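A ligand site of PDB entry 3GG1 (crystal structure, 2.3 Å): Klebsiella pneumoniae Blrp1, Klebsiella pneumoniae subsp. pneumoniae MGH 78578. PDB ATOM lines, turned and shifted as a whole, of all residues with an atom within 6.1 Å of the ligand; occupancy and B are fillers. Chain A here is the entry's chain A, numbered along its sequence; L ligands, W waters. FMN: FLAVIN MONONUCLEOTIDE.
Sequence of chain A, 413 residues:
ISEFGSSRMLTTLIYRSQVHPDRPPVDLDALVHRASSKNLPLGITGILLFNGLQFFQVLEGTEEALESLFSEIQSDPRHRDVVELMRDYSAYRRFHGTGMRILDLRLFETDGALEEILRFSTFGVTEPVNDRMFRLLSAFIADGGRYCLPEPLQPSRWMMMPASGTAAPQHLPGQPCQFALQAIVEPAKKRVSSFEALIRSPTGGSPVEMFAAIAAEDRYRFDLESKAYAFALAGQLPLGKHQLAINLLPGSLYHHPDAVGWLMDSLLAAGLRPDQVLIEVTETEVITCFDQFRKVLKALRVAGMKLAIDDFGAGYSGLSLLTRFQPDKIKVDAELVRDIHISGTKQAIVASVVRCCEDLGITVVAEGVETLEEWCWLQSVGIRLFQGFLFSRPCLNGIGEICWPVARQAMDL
NH1 of Arg 78 is in hydrogen-bond range of O3' of the ligand, 3.2 Å away.
An oxygen (O3P) of the ligand is in salt-bridge range of the guanidinium group (NE) of Arg 34.
The side-chain amide oxygen (OD1) of Asn 39 is in hydrogen-bond range of a nitrogen (N3) of the ligand.
An oxygen (O2') of the ligand sits at hydrogen-bond distance from the side-chain carboxylate of Asp 76 (2.7 Å).
The side-chain amino group (NZ) of Lys 38 lies within salt-bridge range of an oxygen (O2P) of the ligand, at 3.8 Å.
NE2 of Gln 57 lies within hydrogen-bond range of N5 of the ligand.
The side-chain amino group (NZ) of Lys 38 lies within salt-bridge range of the side-chain carboxylate (OE1) of Glu 72 (3.0 Å).
O of Asn 39 lies within hydrogen-bond range of N of Ile 44.
The backbone carbonyl oxygen of Ile 73 is in hydrogen-bond range of a ring nitrogen (NE2) of His 79 (2.7 Å).
OD1 of Asn 39 sits close to O of Ala 35, at 3.5 Å.
The backbone carbonyl oxygen (O) of Ser 17 is in hydrogen-bond range of the backbone NH (N) of Phe 55, at 2.9 Å.
OG of Ser 36 sits at hydrogen-bond distance from N of Met 100, at 3.1 Å.
NE2 of Gln 57 sits close to SD of Met 100.
The side-chain amide nitrogen of Asn 39 sits at hydrogen-bond distance from the backbone carbonyl oxygen of Gly 99 (3.2 Å).
Merely in contact with the ligand: Tyr 15 (3.3 Å), Ala 35 (3.4 Å), Leu 69 (3.4 Å), Ile 73 (3.4 Å), Glu 72 (3.5 Å), Met 100 (3.7 Å), Phe 55 (3.7 Å), His 79 (3.8 Å), Leu 31 (3.8 Å) and Leu 59 (3.9 Å).
Hydrophobic or aromatic side chains that line the ligand: Leu 31, Ala 35, Phe 55, Leu 59, Leu 69, Ile 73, His 79 and Met 100.
The nearest printed residue that does not touch the ligand is Leu 48 (4.1 Å).
Water W3 lies within hydrogen-bond range of the backbone carbonyl oxygen (O) of Leu 31, the backbone NH (N) of Ala 35 and a nitrogen (N1) of the ligand.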
ATOM      1  N   TYR A  15      -5.099  -1.031  16.362  1.00  0.00           N
ATOM      2  CA  TYR A  15      -6.453  -0.918  16.905  1.00  0.00           C
ATOM      3  C   TYR A  15      -6.476  -0.017  18.135  1.00  0.00           C
ATOM      4  O   TYR A  15      -5.428   0.217  18.755  1.00  0.00           O
ATOM      5  CB  TYR A  15      -7.025  -2.303  17.257  1.00  0.00           C
ATOM      6  CG  TYR A  15      -6.422  -2.915  18.504  1.00  0.00           C
ATOM      7  CD1 TYR A  15      -6.935  -2.602  19.757  1.00  0.00           C
ATOM      8  CD2 TYR A  15      -5.336  -3.783  18.422  1.00  0.00           C
ATOM      9  CE1 TYR A  15      -6.377  -3.139  20.909  1.00  0.00           C
ATOM     10  CE2 TYR A  15      -4.777  -4.320  19.574  1.00  0.00           C
ATOM     11  CZ  TYR A  15      -5.297  -4.001  20.807  1.00  0.00           C
ATOM     12  OH  TYR A  15      -4.741  -4.530  21.947  1.00  0.00           O
ATOM     13  N   SER A  17      -8.911   0.468  21.833  1.00  0.00           N
ATOM     14  CA  SER A  17      -9.903  -0.176  22.690  1.00  0.00           C
ATOM     15  C   SER A  17     -10.067   0.610  23.980  1.00  0.00           C
ATOM     16  O   SER A  17      -9.467   1.677  24.130  1.00  0.00           O
ATOM     17  CB  SER A  17      -9.498  -1.635  22.980  1.00  0.00           C
ATOM     18  OG  SER A  17      -8.345  -1.694  23.790  1.00  0.00           O
ATOM     19  N   LEU A  31       1.104  -7.373  32.030  1.00  0.00           N
ATOM     20  CA  LEU A  31       0.540  -7.626  30.704  1.00  0.00           C
ATOM     21  C   LEU A  31       1.563  -7.356  29.614  1.00  0.00           C
ATOM     22  O   LEU A  31       1.746  -8.177  28.712  1.00  0.00           O
ATOM     23  CB  LEU A  31      -0.699  -6.751  30.483  1.00  0.00           C
ATOM     24  CG  LEU A  31      -1.465  -6.924  29.160  1.00  0.00           C
ATOM     25  CD1 LEU A  31      -2.955  -6.768  29.377  1.00  0.00           C
ATOM     26  CD2 LEU A  31      -1.008  -5.944  28.084  1.00  0.00           C
ATOM     27  N   ARG A  34       4.621  -9.836  29.739  1.00  0.00           N
ATOM     28  CA  ARG A  34       4.204 -11.110  29.154  1.00  0.00           C
ATOM     29  C   ARG A  34       4.073 -10.980  27.637  1.00  0.00           C
ATOM     30  O   ARG A  34       4.505 -11.851  26.893  1.00  0.00           O
ATOM     31  CB  ARG A  34       2.901 -11.592  29.790  1.00  0.00           C
ATOM     32  CG  ARG A  34       2.626 -13.077  29.603  1.00  0.00           C
ATOM     33  CD  ARG A  34       1.579 -13.605  30.577  1.00  0.00           C
ATOM     34  NE  ARG A  34       1.397 -15.054  30.437  1.00  0.00           N
ATOM     35  CZ  ARG A  34       2.259 -15.982  30.876  1.00  0.00           C
ATOM     36  NH1 ARG A  34       3.371 -15.632  31.527  1.00  0.00           N
ATOM     37  NH2 ARG A  34       1.992 -17.265  30.681  1.00  0.00           N
ATOM     38  N   ALA A  35       3.482  -9.862  27.185  1.00  0.00           N
ATOM     39  CA  ALA A  35       3.333  -9.581  25.754  1.00  0.00           C
ATOM     40  C   ALA A  35       4.668  -9.506  25.032  1.00  0.00           C
ATOM     41  O   ALA A  35       4.873 -10.177  24.018  1.00  0.00           O
ATOM     42  CB  ALA A  35       2.548  -8.283  25.552  1.00  0.00           C
ATOM     43  N   SER A  36       5.579  -8.683  25.558  1.00  0.00           N
ATOM     44  CA  SER A  36       6.900  -8.512  24.952  1.00  0.00           C
ATOM     45  C   SER A  36       7.654  -9.830  24.845  1.00  0.00           C
ATOM     46  O   SER A  36       8.264 -10.133  23.815  1.00  0.00           O
ATOM     47  CB  SER A  36       7.724  -7.514  25.768  1.00  0.00           C
ATOM     48  OG  SER A  36       8.878  -7.102  25.058  1.00  0.00           O
ATOM     49  N   LYS A  38       6.323 -12.882  24.828  1.00  0.00           N
ATOM     50  CA  LYS A  38       5.648 -13.777  23.887  1.00  0.00           C
ATOM     51  C   LYS A  38       5.832 -13.309  22.443  1.00  0.00           C
ATOM     52  O   LYS A  38       6.073 -14.120  21.550  1.00  0.00           O
ATOM     53  CB  LYS A  38       4.157 -13.894  24.219  1.00  0.00           C
ATOM     54  CG  LYS A  38       3.483 -15.085  23.537  1.00  0.00           C
ATOM     55  CD  LYS A  38       2.026 -15.241  23.984  1.00  0.00           C
ATOM     56  CE  LYS A  38       1.246 -16.152  23.050  1.00  0.00           C
ATOM     57  NZ  LYS A  38      -0.224 -15.887  23.100  1.00  0.00           N
ATOM     58  N   ASN A  39       5.719 -12.002  22.218  1.00  0.00           N
ATOM     59  CA  ASN A  39       5.788 -11.428  20.870  1.00  0.00           C
ATOM     60  C   ASN A  39       7.111 -11.639  20.141  1.00  0.00           C
ATOM     61  O   ASN A  39       7.117 -11.997  18.968  1.00  0.00           O
ATOM     62  CB  ASN A  39       5.485  -9.919  20.901  1.00  0.00           C
ATOM     63  CG  ASN A  39       4.004  -9.610  21.065  1.00  0.00           C
ATOM     64  OD1 ASN A  39       3.163 -10.503  21.022  1.00  0.00           O
ATOM     65  ND2 ASN A  39       3.685  -8.345  21.254  1.00  0.00           N
ATOM     66  N   ILE A  44       7.033 -10.724  16.392  1.00  0.00           N
ATOM     67  CA  ILE A  44       6.046  -9.661  16.553  1.00  0.00           C
ATOM     68  C   ILE A  44       6.667  -8.526  17.350  1.00  0.00           C
ATOM     69  O   ILE A  44       7.343  -8.754  18.339  1.00  0.00           O
ATOM     70  CB  ILE A  44       4.768 -10.168  17.271  1.00  0.00           C
ATOM     71  CG1 ILE A  44       4.098 -11.266  16.441  1.00  0.00           C
ATOM     72  CG2 ILE A  44       3.793  -9.005  17.528  1.00  0.00           C
ATOM     73  CD1 ILE A  44       2.963 -11.976  17.146  1.00  0.00           C
ATOM     74  N   LEU A  48       2.263  -0.055  22.949  1.00  0.00           N
ATOM     75  CA  LEU A  48       0.941   0.136  23.531  1.00  0.00           C
ATOM     76  C   LEU A  48       0.847   1.513  24.169  1.00  0.00           C
ATOM     77  O   LEU A  48       1.686   1.876  24.980  1.00  0.00           O
ATOM     78  CB  LEU A  48       0.666  -0.948  24.583  1.00  0.00           C
ATOM     79  CG  LEU A  48      -0.711  -0.941  25.251  1.00  0.00           C
ATOM     80  CD1 LEU A  48      -1.811  -1.184  24.220  1.00  0.00           C
ATOM     81  CD2 LEU A  48      -0.766  -1.994  26.349  1.00  0.00           C
ATOM     82  N   PHE A  55      -6.827   2.100  25.208  1.00  0.00           N
ATOM     83  CA  PHE A  55      -5.573   1.567  24.692  1.00  0.00           C
ATOM     84  C   PHE A  55      -5.449   1.897  23.209  1.00  0.00           C
ATOM     85  O   PHE A  55      -6.440   2.106  22.518  1.00  0.00           O
ATOM     86  CB  PHE A  55      -5.510   0.048  24.866  1.00  0.00           C
ATOM     87  CG  PHE A  55      -5.529  -0.391  26.289  1.00  0.00           C
ATOM     88  CD1 PHE A  55      -4.408  -0.235  27.092  1.00  0.00           C
ATOM     89  CD2 PHE A  55      -6.668  -0.968  26.842  1.00  0.00           C
ATOM     90  CE1 PHE A  55      -4.422  -0.641  28.422  1.00  0.00           C
ATOM     91  CE2 PHE A  55      -6.686  -1.376  28.162  1.00  0.00           C
ATOM     92  CZ  PHE A  55      -5.558  -1.213  28.951  1.00  0.00           C
ATOM     93  N   GLN A  57      -2.799   0.197  20.264  1.00  0.00           N
ATOM     94  CA  GLN A  57      -1.700  -0.739  20.050  1.00  0.00           C
ATOM     95  C   GLN A  57      -1.300  -0.865  18.587  1.00  0.00           C
ATOM     96  O   GLN A  57      -2.156  -0.966  17.702  1.00  0.00           O
ATOM     97  CB  GLN A  57      -2.066  -2.122  20.609  1.00  0.00           C
ATOM     98  CG  GLN A  57      -0.861  -3.050  20.711  1.00  0.00           C
ATOM     99  CD  GLN A  57      -1.147  -4.299  21.497  1.00  0.00           C
ATOM    100  OE1 GLN A  57      -2.244  -4.848  21.437  1.00  0.00           O
ATOM    101  NE2 GLN A  57      -0.157  -4.763  22.235  1.00  0.00           N
ATOM    102  N   LEU A  59       0.918  -3.336  16.089  1.00  0.00           N
ATOM    103  CA  LEU A  59       1.488  -4.668  15.974  1.00  0.00           C
ATOM    104  C   LEU A  59       2.100  -4.877  14.602  1.00  0.00           C
ATOM    105  O   LEU A  59       1.475  -4.576  13.582  1.00  0.00           O
ATOM    106  CB  LEU A  59       0.415  -5.739  16.218  1.00  0.00           C
ATOM    107  CG  LEU A  59      -0.165  -5.821  17.622  1.00  0.00           C
ATOM    108  CD1 LEU A  59      -1.393  -6.718  17.630  1.00  0.00           C
ATOM    109  CD2 LEU A  59       0.875  -6.327  18.619  1.00  0.00           C
ATOM    110  N   LEU A  69      -2.687 -13.549  16.946  1.00  0.00           N
ATOM    111  CA  LEU A  69      -2.561 -12.713  18.135  1.00  0.00           C
ATOM    112  C   LEU A  69      -3.788 -11.812  18.357  1.00  0.00           C
ATOM    113  O   LEU A  69      -4.298 -11.711  19.466  1.00  0.00           O
ATOM    114  CB  LEU A  69      -1.279 -11.868  18.085  1.00  0.00           C
ATOM    115  CG  LEU A  69      -1.082 -10.836  19.201  1.00  0.00           C
ATOM    116  CD1 LEU A  69      -1.147 -11.475  20.581  1.00  0.00           C
ATOM    117  CD2 LEU A  69       0.225 -10.087  19.031  1.00  0.00           C
ATOM    118  N   GLU A  72      -6.873 -13.493  19.823  1.00  0.00           N
ATOM    119  CA  GLU A  72      -6.770 -13.603  21.282  1.00  0.00           C
ATOM    120  C   GLU A  72      -7.097 -12.274  21.936  1.00  0.00           C
ATOM    121  O   GLU A  72      -7.900 -12.206  22.874  1.00  0.00           O
ATOM    122  CB  GLU A  72      -5.365 -14.047  21.698  1.00  0.00           C
ATOM    123  CG  GLU A  72      -4.901 -15.360  21.100  1.00  0.00           C
ATOM    124  CD  GLU A  72      -3.772 -15.992  21.896  1.00  0.00           C
ATOM    125  OE1 GLU A  72      -2.631 -16.038  21.393  1.00  0.00           O
ATOM    126  OE2 GLU A  72      -4.046 -16.437  23.033  1.00  0.00           O
ATOM    127  N   ILE A  73      -6.481 -11.206  21.434  1.00  0.00           N
ATOM    128  CA  ILE A  73      -6.684  -9.854  21.976  1.00  0.00           C
ATOM    129  C   ILE A  73      -8.148  -9.431  21.897  1.00  0.00           C
ATOM    130  O   ILE A  73      -8.659  -8.814  22.835  1.00  0.00           O
ATOM    131  CB  ILE A  73      -5.770  -8.819  21.267  1.00  0.00           C
ATOM    132  CG1 ILE A  73      -4.308  -9.080  21.639  1.00  0.00           C
ATOM    133  CG2 ILE A  73      -6.161  -7.395  21.668  1.00  0.00           C
ATOM    134  CD1 ILE A  73      -3.314  -8.324  20.782  1.00  0.00           C
ATOM    135  N   GLN A  74      -8.825  -9.757  20.797  1.00  0.00           N
ATOM    136  CA  GLN A  74     -10.247  -9.466  20.631  1.00  0.00           C
ATOM    137  C   GLN A  74     -11.121 -10.170  21.673  1.00  0.00           C
ATOM    138  O   GLN A  74     -12.141  -9.635  22.095  1.00  0.00           O
ATOM    139  CB  GLN A  74     -10.726  -9.880  19.230  1.00  0.00           C
ATOM    140  CG  GLN A  74     -10.494  -8.839  18.157  1.00  0.00           C
ATOM    141  CD  GLN A  74     -11.072  -9.268  16.815  1.00  0.00           C
ATOM    142  OE1 GLN A  74     -10.939 -10.426  16.413  1.00  0.00           O
ATOM    143  NE2 GLN A  74     -11.704  -8.342  16.113  1.00  0.00           N
ATOM    144  N   ASP A  76     -10.136 -10.933  24.687  1.00  0.00           N
ATOM    145  CA  ASP A  76      -9.609 -10.637  26.017  1.00  0.00           C
ATOM    146  C   ASP A  76     -10.601  -9.789  26.834  1.00  0.00           C
ATOM    147  O   ASP A  76     -10.955  -8.682  26.430  1.00  0.00           O
ATOM    148  CB  ASP A  76      -8.268  -9.911  25.894  1.00  0.00           C
ATOM    149  CG  ASP A  76      -7.487  -9.898  27.187  1.00  0.00           C
ATOM    150  OD1 ASP A  76      -8.097  -9.701  28.249  1.00  0.00           O
ATOM    151  OD2 ASP A  76      -6.254 -10.073  27.129  1.00  0.00           O
ATOM    152  N   ARG A  78     -10.111  -8.128  29.518  1.00  0.00           N
ATOM    153  CA  ARG A  78      -9.477  -6.955  30.152  1.00  0.00           C
ATOM    154  C   ARG A  78      -9.848  -5.638  29.468  1.00  0.00           C
ATOM    155  O   ARG A  78      -9.636  -4.561  30.043  1.00  0.00           O
ATOM    156  CB  ARG A  78      -7.951  -7.093  30.135  1.00  0.00           C
ATOM    157  CG  ARG A  78      -7.370  -8.128  31.102  1.00  0.00           C
ATOM    158  CD  ARG A  78      -6.382  -9.037  30.384  1.00  0.00           C
ATOM    159  NE  ARG A  78      -5.164  -9.328  31.117  1.00  0.00           N
ATOM    160  CZ  ARG A  78      -4.137  -9.995  30.599  1.00  0.00           C
ATOM    161  NH1 ARG A  78      -4.171 -10.441  29.337  1.00  0.00           N
ATOM    162  NH2 ARG A  78      -3.051 -10.222  31.324  1.00  0.00           N
ATOM    163  N   HIS A  79     -10.369  -5.709  28.244  1.00  0.00           N
ATOM    164  CA  HIS A  79     -10.793  -4.513  27.504  1.00  0.00           C
ATOM    165  C   HIS A  79     -12.021  -4.788  26.642  1.00  0.00           C
ATOM    166  O   HIS A  79     -12.493  -5.921  26.546  1.00  0.00           O
ATOM    167  CB  HIS A  79      -9.622  -3.962  26.675  1.00  0.00           C
ATOM    168  CG  HIS A  79      -9.195  -4.831  25.534  1.00  0.00           C
ATOM    169  ND1 HIS A  79      -8.332  -4.391  24.545  1.00  0.00           N
ATOM    170  CD2 HIS A  79      -9.494  -6.118  25.212  1.00  0.00           C
ATOM    171  CE1 HIS A  79      -8.124  -5.361  23.672  1.00  0.00           C
ATOM    172  NE2 HIS A  79      -8.819  -6.418  24.060  1.00  0.00           N
ATOM    173  N   GLY A  99       9.525  -6.192  21.485  1.00  0.00           N
ATOM    174  CA  GLY A  99       8.394  -7.111  21.505  1.00  0.00           C
ATOM    175  C   GLY A  99       7.107  -6.368  21.789  1.00  0.00           C
ATOM    176  O   GLY A  99       6.179  -6.380  20.978  1.00  0.00           O
ATOM    177  N   MET A 100       7.063  -5.716  22.943  1.00  0.00           N
ATOM    178  CA  MET A 100       5.972  -4.825  23.292  1.00  0.00           C
ATOM    179  C   MET A 100       6.443  -3.846  24.354  1.00  0.00           C
ATOM    180  O   MET A 100       7.338  -4.154  25.140  1.00  0.00           O
ATOM    181  CB  MET A 100       4.757  -5.616  23.781  1.00  0.00           C
ATOM    182  CG  MET A 100       3.493  -4.773  24.006  1.00  0.00           C
ATOM    183  SD  MET A 100       3.040  -3.682  22.639  1.00  0.00           S
ATOM    184  CE  MET A 100       3.068  -4.809  21.245  1.00  0.00           C
HETATM  185  N1  FMN L   1      -0.764 -10.643  24.296  1.00  0.00           N
HETATM  186  C2  FMN L   1       0.379 -10.877  23.571  1.00  0.00           C
HETATM  187  O2  FMN L   1       0.837 -12.016  23.534  1.00  0.00           O
HETATM  188  N3  FMN L   1       0.999  -9.843  22.901  1.00  0.00           N
HETATM  189  C4  FMN L   1       0.448  -8.578  22.936  1.00  0.00           C
HETATM  190  O4  FMN L   1       0.983  -7.680  22.278  1.00  0.00           O
HETATM  191  C4A FMN L   1      -0.710  -8.331  23.675  1.00  0.00           C
HETATM  192  N5  FMN L   1      -1.270  -7.068  23.746  1.00  0.00           N
HETATM  193  C5A FMN L   1      -2.426  -6.855  24.469  1.00  0.00           C
HETATM  194  C6  FMN L   1      -2.967  -5.575  24.530  1.00  0.00           C
HETATM  195  C7  FMN L   1      -4.128  -5.330  25.260  1.00  0.00           C
HETATM  196  C7M FMN L   1      -4.605  -3.914  25.402  1.00  0.00           C
HETATM  197  C8  FMN L   1      -4.736  -6.383  25.940  1.00  0.00           C
HETATM  198  C8M FMN L   1      -5.877  -6.145  26.890  1.00  0.00           C
HETATM  199  C9  FMN L   1      -4.208  -7.674  25.875  1.00  0.00           C
HETATM  200  C9A FMN L   1      -3.031  -7.907  25.158  1.00  0.00           C
HETATM  201  N10 FMN L   1      -2.471  -9.189  25.091  1.00  0.00           N
HETATM  202  C10 FMN L   1      -1.318  -9.384  24.355  1.00  0.00           C
HETATM  203  C1' FMN L   1      -2.975 -10.338  25.924  1.00  0.00           C
HETATM  204  C2' FMN L   1      -3.764 -11.308  25.048  1.00  0.00           C
HETATM  205  O2' FMN L   1      -5.080 -10.823  24.852  1.00  0.00           O
HETATM  206  C3' FMN L   1      -3.845 -12.701  25.670  1.00  0.00           C
HETATM  207  O3' FMN L   1      -4.243 -12.598  27.018  1.00  0.00           O
HETATM  208  C4' FMN L   1      -2.526 -13.470  25.616  1.00  0.00           C
HETATM  209  O4' FMN L   1      -1.915 -13.340  24.354  1.00  0.00           O
HETATM  210  C5' FMN L   1      -2.790 -14.952  25.910  1.00  0.00           C
HETATM  211  O5' FMN L   1      -1.597 -15.696  25.756  1.00  0.00           O
HETATM  212  P   FMN L   1      -0.949 -16.448  27.024  1.00  0.00           P
HETATM  213  O1P FMN L   1      -1.887 -17.562  27.433  1.00  0.00           O
HETATM  214  O2P FMN L   1       0.399 -17.019  26.644  1.00  0.00           O
HETATM  215  O3P FMN L   1      -0.786 -15.463  28.150  1.00  0.00           O
HETATM  216  O   HOH W   1      -6.879 -13.595  26.745  1.00  0.00           O
HETATM  217  O   HOH W   2       1.073 -12.415  26.378  1.00  0.00           O
HETATM  218  O   HOH W   3       0.090 -10.256  27.627  1.00  0.00           O
HETATM  219  O   HOH W   4       0.313 -19.270  24.412  1.00  0.00           O
